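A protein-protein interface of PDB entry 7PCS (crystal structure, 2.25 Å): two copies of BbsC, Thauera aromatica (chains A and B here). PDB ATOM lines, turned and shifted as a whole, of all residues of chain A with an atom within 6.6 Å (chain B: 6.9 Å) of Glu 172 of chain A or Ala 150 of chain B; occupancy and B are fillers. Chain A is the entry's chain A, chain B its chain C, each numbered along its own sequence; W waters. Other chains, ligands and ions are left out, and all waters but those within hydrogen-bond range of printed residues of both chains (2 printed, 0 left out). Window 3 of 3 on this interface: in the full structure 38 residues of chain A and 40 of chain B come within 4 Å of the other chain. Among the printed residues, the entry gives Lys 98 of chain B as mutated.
The side-chain carboxylate (OE2) of Glu 172 of chain A is in hydrogen-bond range of the backbone NH (N) of Leu 100 of chain B (2.6 Å). The side-chain carboxylate (OE1) of Glu 172 of chain A is in hydrogen-bond range of the backbone NH (N) of Asn 151 of chain B.
The backbone NH of Lys 98 of chain B lies within hydrogen-bond range of the backbone carbonyl oxygen of Asn 151 of chain B (3.4 Å). O of Leu 149 of chain B is in hydrogen-bond range of OG1 of Thr 152 of chain B, 2.6 Å away. The guanidinium group (NH1) of Arg 131 of chain A sits close to the backbone carbonyl oxygen (O) of Glu 172 of chain A (3.5 Å). O of Leu 169 of chain A is in hydrogen-bond range of OG of Ser 173 of chain A.
Among the printed residues, merely in contact across the chains: Ala 168 of chain A with Leu 149 of chain B (3.3 Å), Leu 169 of chain A with Ser 153 of chain B (3.5 Å), Leu 171 of chain A with Gly 148 of chain B (3.5 Å), Glu 172 of chain A with Pro 99 of chain B (3.6 Å), Ala 168 of chain A with Gly 148 of chain B (3.6 Å), Ala 168 of chain A with Ser 153 of chain B (3.8 Å), Ala 168 of chain A with Ala 150 of chain B (3.8 Å), Leu 171 of chain A with Leu 149 of chain B (3.8 Å), Leu 171 of chain A with Ala 150 of chain B (3.9 Å), Glu 172 of chain A with Ala 150 of chain B (3.9 Å), Ala 168 of chain A with Thr 152 of chain B (3.9 Å) and Leu 169 of chain A with Leu 100 of chain B (3.9 Å).
Printed residues of chain B within 4 Å of Ala 168 of chain A: Gly 148 (3.6 Å), Leu 149 (3.3 Å), Ala 150 (3.8 Å), Thr 152 (3.9 Å) and Ser 153 (3.8 Å). Of the printed residues of chain B, Leu 169 of chain A touches Leu 100 and Ser 153. Ala 170 of chain A touches none of the printed residues of chain B. Of the printed residues of chain A, Pro 99 of chain B touches Glu 172. Of the printed residues of chain A, Gly 148 of chain B touches Ala 168 (3.6 Å) and Leu 171 (3.5 Å). Ala 150 of chain B touches three residues of chain A. Printed residues of chain A within 4 Å of Thr 152 of chain B: Ala 168 (3.9 Å). Ser 154 of chain B touches none of the printed residues of chain A. The nearest residue of chain A that does not touch Ala 150 of chain B is Arg 167 of chain A (5.5 Å). The nearest printed residue of chain A that does not touch Pro 99 of chain B is Arg 131 of chain A (6.6 Å).
Printed residues of chain A that touch a printed residue of chain B: Ala 168, Leu 169, Leu 171 and Glu 172. Hydrophobic or aromatic side chains of chain A that line the printed part of chain B: Ala 168, Leu 169 and Leu 171. Of the 13 printed residues of chain B, 8 touch a printed residue of chain A. Hydrophobic or aromatic side chains of chain B within 4 Å of the printed part of chain A: Leu 100 and Ala 150.
No position is printed for both chains.
Water W2 lies within hydrogen-bond range of OE1 of Glu 172 of chain A (2.4 Å), OG of Ser 153 of chain B (2.6 Å), O of Lys 98 of chain B (2.8 Å), N of Thr 152 of chain B (3.3 Å) and N of Leu 100 of chain B (3.3 Å). Water W1 bridges the backbone carbonyl oxygen (O) of Gly 148 of chain B (2.6 Å) and the guanidinium group (NH2) of Arg 167 of chain A (3.0 Å).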
ATOM      1  N   ARG A 131      16.100  11.783 -17.610  1.00  0.00           N
ATOM      2  CA  ARG A 131      16.118  13.196 -17.243  1.00  0.00           C
ATOM      3  C   ARG A 131      15.669  13.394 -15.798  1.00  0.00           C
ATOM      4  O   ARG A 131      16.190  14.264 -15.088  1.00  0.00           O
ATOM      5  CB  ARG A 131      15.217  13.984 -18.193  1.00  0.00           C
ATOM      6  CG  ARG A 131      15.622  13.907 -19.658  1.00  0.00           C
ATOM      7  CD  ARG A 131      14.728  14.802 -20.509  1.00  0.00           C
ATOM      8  NE  ARG A 131      14.769  16.193 -20.069  1.00  0.00           N
ATOM      9  CZ  ARG A 131      14.001  17.156 -20.564  1.00  0.00           C
ATOM     10  NH1 ARG A 131      13.131  16.916 -21.533  1.00  0.00           N
ATOM     11  NH2 ARG A 131      14.103  18.388 -20.070  1.00  0.00           N
ATOM     12  N   ARG A 167      19.814  13.645 -32.423  1.00  0.00           N
ATOM     13  CA  ARG A 167      20.287  15.001 -32.165  1.00  0.00           C
ATOM     14  C   ARG A 167      19.185  15.872 -31.572  1.00  0.00           C
ATOM     15  O   ARG A 167      19.453  16.708 -30.702  1.00  0.00           O
ATOM     16  CB  ARG A 167      20.829  15.605 -33.460  1.00  0.00           C
ATOM     17  CG  ARG A 167      22.175  14.994 -33.916  1.00  0.00           C
ATOM     18  CD  ARG A 167      22.421  15.247 -35.391  1.00  0.00           C
ATOM     19  NE  ARG A 167      22.420  16.673 -35.686  1.00  0.00           N
ATOM     20  CZ  ARG A 167      23.513  17.381 -35.918  1.00  0.00           C
ATOM     21  NH1 ARG A 167      24.710  16.815 -35.931  1.00  0.00           N
ATOM     22  NH2 ARG A 167      23.406  18.687 -36.141  1.00  0.00           N
ATOM     23  N   ALA A 168      17.939  15.690 -32.016  1.00  0.00           N
ATOM     24  CA  ALA A 168      16.831  16.443 -31.433  1.00  0.00           C
ATOM     25  C   ALA A 168      16.711  16.171 -29.938  1.00  0.00           C
ATOM     26  O   ALA A 168      16.640  17.100 -29.124  1.00  0.00           O
ATOM     27  CB  ALA A 168      15.528  16.100 -32.150  1.00  0.00           C
ATOM     28  N   LEU A 169      16.690  14.895 -29.557  1.00  0.00           N
ATOM     29  CA  LEU A 169      16.552  14.541 -28.151  1.00  0.00           C
ATOM     30  C   LEU A 169      17.829  14.815 -27.364  1.00  0.00           C
ATOM     31  O   LEU A 169      17.765  15.075 -26.157  1.00  0.00           O
ATOM     32  CB  LEU A 169      16.162  13.073 -28.029  1.00  0.00           C
ATOM     33  CG  LEU A 169      14.800  12.705 -28.619  1.00  0.00           C
ATOM     34  CD1 LEU A 169      14.497  11.246 -28.402  1.00  0.00           C
ATOM     35  CD2 LEU A 169      13.713  13.583 -27.995  1.00  0.00           C
ATOM     36  N   ALA A 170      18.993  14.749 -28.009  1.00  0.00           N
ATOM     37  CA  ALA A 170      20.213  15.179 -27.341  1.00  0.00           C
ATOM     38  C   ALA A 170      20.059  16.601 -26.824  1.00  0.00           C
ATOM     39  O   ALA A 170      20.348  16.893 -25.657  1.00  0.00           O
ATOM     40  CB  ALA A 170      21.399  15.085 -28.300  1.00  0.00           C
ATOM     41  N   LEU A 171      19.595  17.502 -27.690  1.00  0.00           N
ATOM     42  CA  LEU A 171      19.404  18.889 -27.284  1.00  0.00           C
ATOM     43  C   LEU A 171      18.271  19.018 -26.277  1.00  0.00           C
ATOM     44  O   LEU A 171      18.374  19.794 -25.321  1.00  0.00           O
ATOM     45  CB  LEU A 171      19.126  19.755 -28.511  1.00  0.00           C
ATOM     46  CG  LEU A 171      20.316  20.050 -29.419  1.00  0.00           C
ATOM     47  CD1 LEU A 171      19.856  20.616 -30.740  1.00  0.00           C
ATOM     48  CD2 LEU A 171      21.253  21.027 -28.706  1.00  0.00           C
ATOM     49  N   GLU A 172      17.192  18.252 -26.457  1.00  0.00           N
ATOM     50  CA  GLU A 172      16.037  18.393 -25.578  1.00  0.00           C
ATOM     51  C   GLU A 172      16.345  17.932 -24.160  1.00  0.00           C
ATOM     52  O   GLU A 172      15.766  18.451 -23.199  1.00  0.00           O
ATOM     53  CB  GLU A 172      14.850  17.608 -26.137  1.00  0.00           C
ATOM     54  CG  GLU A 172      13.519  18.015 -25.555  1.00  0.00           C
ATOM     55  CD  GLU A 172      12.342  17.323 -26.227  1.00  0.00           C
ATOM     56  OE1 GLU A 172      12.312  17.258 -27.473  1.00  0.00           O
ATOM     57  OE2 GLU A 172      11.442  16.850 -25.507  1.00  0.00           O
ATOM     58  N   SER A 173      17.245  16.968 -24.007  1.00  0.00           N
ATOM     59  CA  SER A 173      17.522  16.372 -22.712  1.00  0.00           C
ATOM     60  C   SER A 173      18.838  16.827 -22.112  1.00  0.00           C
ATOM     61  O   SER A 173      19.143  16.439 -20.980  1.00  0.00           O
ATOM     62  CB  SER A 173      17.543  14.848 -22.834  1.00  0.00           C
ATOM     63  OG  SER A 173      18.588  14.439 -23.706  1.00  0.00           O
ATOM     64  N   ALA A 174      19.619  17.637 -22.834  1.00  0.00           N
ATOM     65  CA  ALA A 174      20.990  17.915 -22.421  1.00  0.00           C
ATOM     66  C   ALA A 174      21.059  18.440 -20.994  1.00  0.00           C
ATOM     67  O   ALA A 174      21.938  18.047 -20.222  1.00  0.00           O
ATOM     68  CB  ALA A 174      21.635  18.914 -23.385  1.00  0.00           C
ATOM     69  N   ARG A 175      20.139  19.321 -20.615  1.00  0.00           N
ATOM     70  CA  ARG A 175      20.278  19.992 -19.328  1.00  0.00           C
ATOM     71  C   ARG A 175      20.169  19.030 -18.150  1.00  0.00           C
ATOM     72  O   ARG A 175      20.614  19.372 -17.049  1.00  0.00           O
ATOM     73  CB  ARG A 175      19.216  21.083 -19.177  1.00  0.00           C
ATOM     74  CG  ARG A 175      19.626  22.255 -18.280  1.00  0.00           C
ATOM     75  CD  ARG A 175      18.795  23.502 -18.615  1.00  0.00           C
ATOM     76  NE  ARG A 175      19.574  24.736 -18.642  1.00  0.00           N
ATOM     77  CZ  ARG A 175      19.994  25.317 -19.757  1.00  0.00           C
ATOM     78  NH1 ARG A 175      19.728  24.800 -20.946  1.00  0.00           N
ATOM     79  NH2 ARG A 175      20.704  26.439 -19.680  1.00  0.00           N
ATOM     80  N   ASP A 176      19.597  17.844 -18.349  1.00  0.00           N
ATOM     81  CA  ASP A 176      19.316  16.910 -17.263  1.00  0.00           C
ATOM     82  C   ASP A 176      20.265  15.713 -17.262  1.00  0.00           C
ATOM     83  O   ASP A 176      19.871  14.588 -16.947  1.00  0.00           O
ATOM     84  CB  ASP A 176      17.872  16.427 -17.336  1.00  0.00           C
ATOM     85  CG  ASP A 176      16.876  17.561 -17.219  1.00  0.00           C
ATOM     86  OD1 ASP A 176      17.163  18.535 -16.488  1.00  0.00           O
ATOM     87  OD2 ASP A 176      15.803  17.479 -17.854  1.00  0.00           O
ATOM     88  N   ALA B  97       5.886  20.280 -34.234  1.00  0.00           N
ATOM     89  CA  ALA B  97       6.963  19.955 -33.308  1.00  0.00           C
ATOM     90  C   ALA B  97       6.493  20.177 -31.876  1.00  0.00           C
ATOM     91  O   ALA B  97       5.874  21.201 -31.572  1.00  0.00           O
ATOM     92  CB  ALA B  97       8.194  20.813 -33.589  1.00  0.00           C
ATOM     93  N   LYS B  98       6.768  19.213 -31.001  1.00  0.00           N
ATOM     94  CA  LYS B  98       6.349  19.332 -29.612  1.00  0.00           C
ATOM     95  C   LYS B  98       7.365  18.660 -28.706  1.00  0.00           C
ATOM     96  O   LYS B  98       8.057  17.729 -29.137  1.00  0.00           O
ATOM     97  CB  LYS B  98       4.974  18.706 -29.355  1.00  0.00           C
ATOM     98  CG  LYS B  98       4.182  18.354 -30.577  1.00  0.00           C
ATOM     99  CD  LYS B  98       2.800  17.859 -30.165  1.00  0.00           C
ATOM    100  CE  LYS B  98       2.090  17.167 -31.311  1.00  0.00           C
ATOM    101  NZ  LYS B  98       0.623  17.004 -31.026  1.00  0.00           N
ATOM    102  N   PRO B  99       7.482  19.108 -27.451  1.00  0.00           N
ATOM    103  CA  PRO B  99       8.358  18.411 -26.497  1.00  0.00           C
ATOM    104  C   PRO B  99       7.995  16.939 -26.424  1.00  0.00           C
ATOM    105  O   PRO B  99       6.844  16.557 -26.631  1.00  0.00           O
ATOM    106  CB  PRO B  99       8.096  19.120 -25.164  1.00  0.00           C
ATOM    107  CG  PRO B  99       7.509  20.457 -25.529  1.00  0.00           C
ATOM    108  CD  PRO B  99       6.836  20.301 -26.873  1.00  0.00           C
ATOM    109  N   LEU B 100       8.997  16.115 -26.123  1.00  0.00           N
ATOM    110  CA  LEU B 100       8.812  14.666 -26.039  1.00  0.00           C
ATOM    111  C   LEU B 100       7.573  14.250 -25.259  1.00  0.00           C
ATOM    112  O   LEU B 100       6.836  13.382 -25.746  1.00  0.00           O
ATOM    113  CB  LEU B 100      10.077  14.052 -25.422  1.00  0.00           C
ATOM    114  CG  LEU B 100      10.277  12.543 -25.541  1.00  0.00           C
ATOM    115  CD1 LEU B 100      10.192  12.108 -26.988  1.00  0.00           C
ATOM    116  CD2 LEU B 100      11.635  12.152 -24.938  1.00  0.00           C
ATOM    117  N   PRO B 101       7.289  14.799 -24.074  1.00  0.00           N
ATOM    118  CA  PRO B 101       6.116  14.315 -23.318  1.00  0.00           C
ATOM    119  C   PRO B 101       4.803  14.453 -24.069  1.00  0.00           C
ATOM    120  O   PRO B 101       3.902  13.621 -23.900  1.00  0.00           O
ATOM    121  CB  PRO B 101       6.125  15.185 -22.050  1.00  0.00           C
ATOM    122  CG  PRO B 101       7.558  15.673 -21.923  1.00  0.00           C
ATOM    123  CD  PRO B 101       8.026  15.856 -23.350  1.00  0.00           C
ATOM    124  N   ILE B 103       4.247  14.011 -27.125  1.00  0.00           N
ATOM    125  CA  ILE B 103       4.233  13.175 -28.320  1.00  0.00           C
ATOM    126  C   ILE B 103       3.547  11.855 -27.992  1.00  0.00           C
ATOM    127  O   ILE B 103       3.970  11.126 -27.088  1.00  0.00           O
ATOM    128  CB  ILE B 103       5.655  12.946 -28.852  1.00  0.00           C
ATOM    129  CG1 ILE B 103       6.338  14.295 -29.082  1.00  0.00           C
ATOM    130  CG2 ILE B 103       5.618  12.158 -30.141  1.00  0.00           C
ATOM    131  CD1 ILE B 103       7.747  14.195 -29.661  1.00  0.00           C
ATOM    132  N   GLY B 148      17.628  18.070 -36.321  1.00  0.00           N
ATOM    133  CA  GLY B 148      17.348  17.754 -34.936  1.00  0.00           C
ATOM    134  C   GLY B 148      17.519  18.941 -34.015  1.00  0.00           C
ATOM    135  O   GLY B 148      18.638  19.421 -33.810  1.00  0.00           O
ATOM    136  N   LEU B 149      16.411  19.428 -33.465  1.00  0.00           N
ATOM    137  CA  LEU B 149      16.428  20.500 -32.486  1.00  0.00           C
ATOM    138  C   LEU B 149      15.569  20.102 -31.297  1.00  0.00           C
ATOM    139  O   LEU B 149      14.730  19.205 -31.386  1.00  0.00           O
ATOM    140  CB  LEU B 149      15.917  21.809 -33.086  1.00  0.00           C
ATOM    141  CG  LEU B 149      16.731  22.399 -34.237  1.00  0.00           C
ATOM    142  CD1 LEU B 149      15.863  23.433 -34.974  1.00  0.00           C
ATOM    143  CD2 LEU B 149      18.024  23.006 -33.770  1.00  0.00           C
ATOM    144  N   ALA B 150      15.787  20.781 -30.176  1.00  0.00           N
ATOM    145  CA  ALA B 150      14.977  20.516 -28.997  1.00  0.00           C
ATOM    146  C   ALA B 150      13.502  20.694 -29.328  1.00  0.00           C
ATOM    147  O   ALA B 150      13.119  21.633 -30.032  1.00  0.00           O
ATOM    148  CB  ALA B 150      15.377  21.455 -27.862  1.00  0.00           C
ATOM    149  N   ASN B 151      12.679  19.767 -28.834  1.00  0.00           N
ATOM    150  CA  ASN B 151      11.230  19.839 -28.997  1.00  0.00           C
ATOM    151  C   ASN B 151      10.830  19.750 -30.463  1.00  0.00           C
ATOM    152  O   ASN B 151       9.925  20.451 -30.918  1.00  0.00           O
ATOM    153  CB  ASN B 151      10.671  21.113 -28.360  1.00  0.00           C
ATOM    154  CG  ASN B 151      11.196  21.341 -26.949  1.00  0.00           C
ATOM    155  OD1 ASN B 151      11.040  20.496 -26.063  1.00  0.00           O
ATOM    156  ND2 ASN B 151      11.838  22.478 -26.739  1.00  0.00           N
ATOM    157  N   THR B 152      11.515  18.885 -31.212  1.00  0.00           N
ATOM    158  CA  THR B 152      11.138  18.610 -32.593  1.00  0.00           C
ATOM    159  C   THR B 152      11.308  17.138 -32.952  1.00  0.00           C
ATOM    160  O   THR B 152      11.243  16.797 -34.142  1.00  0.00           O
ATOM    161  CB  THR B 152      11.965  19.461 -33.576  1.00  0.00           C
ATOM    162  OG1 THR B 152      13.338  19.053 -33.525  1.00  0.00           O
ATOM    163  CG2 THR B 152      11.860  20.941 -33.247  1.00  0.00           C
ATOM    164  N   SER B 153      11.496  16.254 -31.966  1.00  0.00           N
ATOM    165  CA  SER B 153      11.939  14.889 -32.249  1.00  0.00           C
ATOM    166  C   SER B 153      11.043  14.196 -33.267  1.00  0.00           C
ATOM    167  O   SER B 153      11.534  13.501 -34.168  1.00  0.00           O
ATOM    168  CB  SER B 153      11.997  14.081 -30.949  1.00  0.00           C
ATOM    169  OG  SER B 153      10.792  14.217 -30.211  1.00  0.00           O
ATOM    170  N   SER B 154       9.723  14.358 -33.133  1.00  0.00           N
ATOM    171  CA  SER B 154       8.809  13.689 -34.051  1.00  0.00           C
ATOM    172  C   SER B 154       8.900  14.274 -35.453  1.00  0.00           C
ATOM    173  O   SER B 154       8.755  13.546 -36.438  1.00  0.00           O
ATOM    174  CB  SER B 154       7.371  13.774 -33.535  1.00  0.00           C
ATOM    175  OG  SER B 154       6.927  15.113 -33.427  1.00  0.00           O
HETATM  176  O   HOH W   1      21.024  19.972 -34.748  1.00  0.00           O
HETATM  177  O   HOH W   2      10.573  16.555 -29.031  1.00  0.00           O
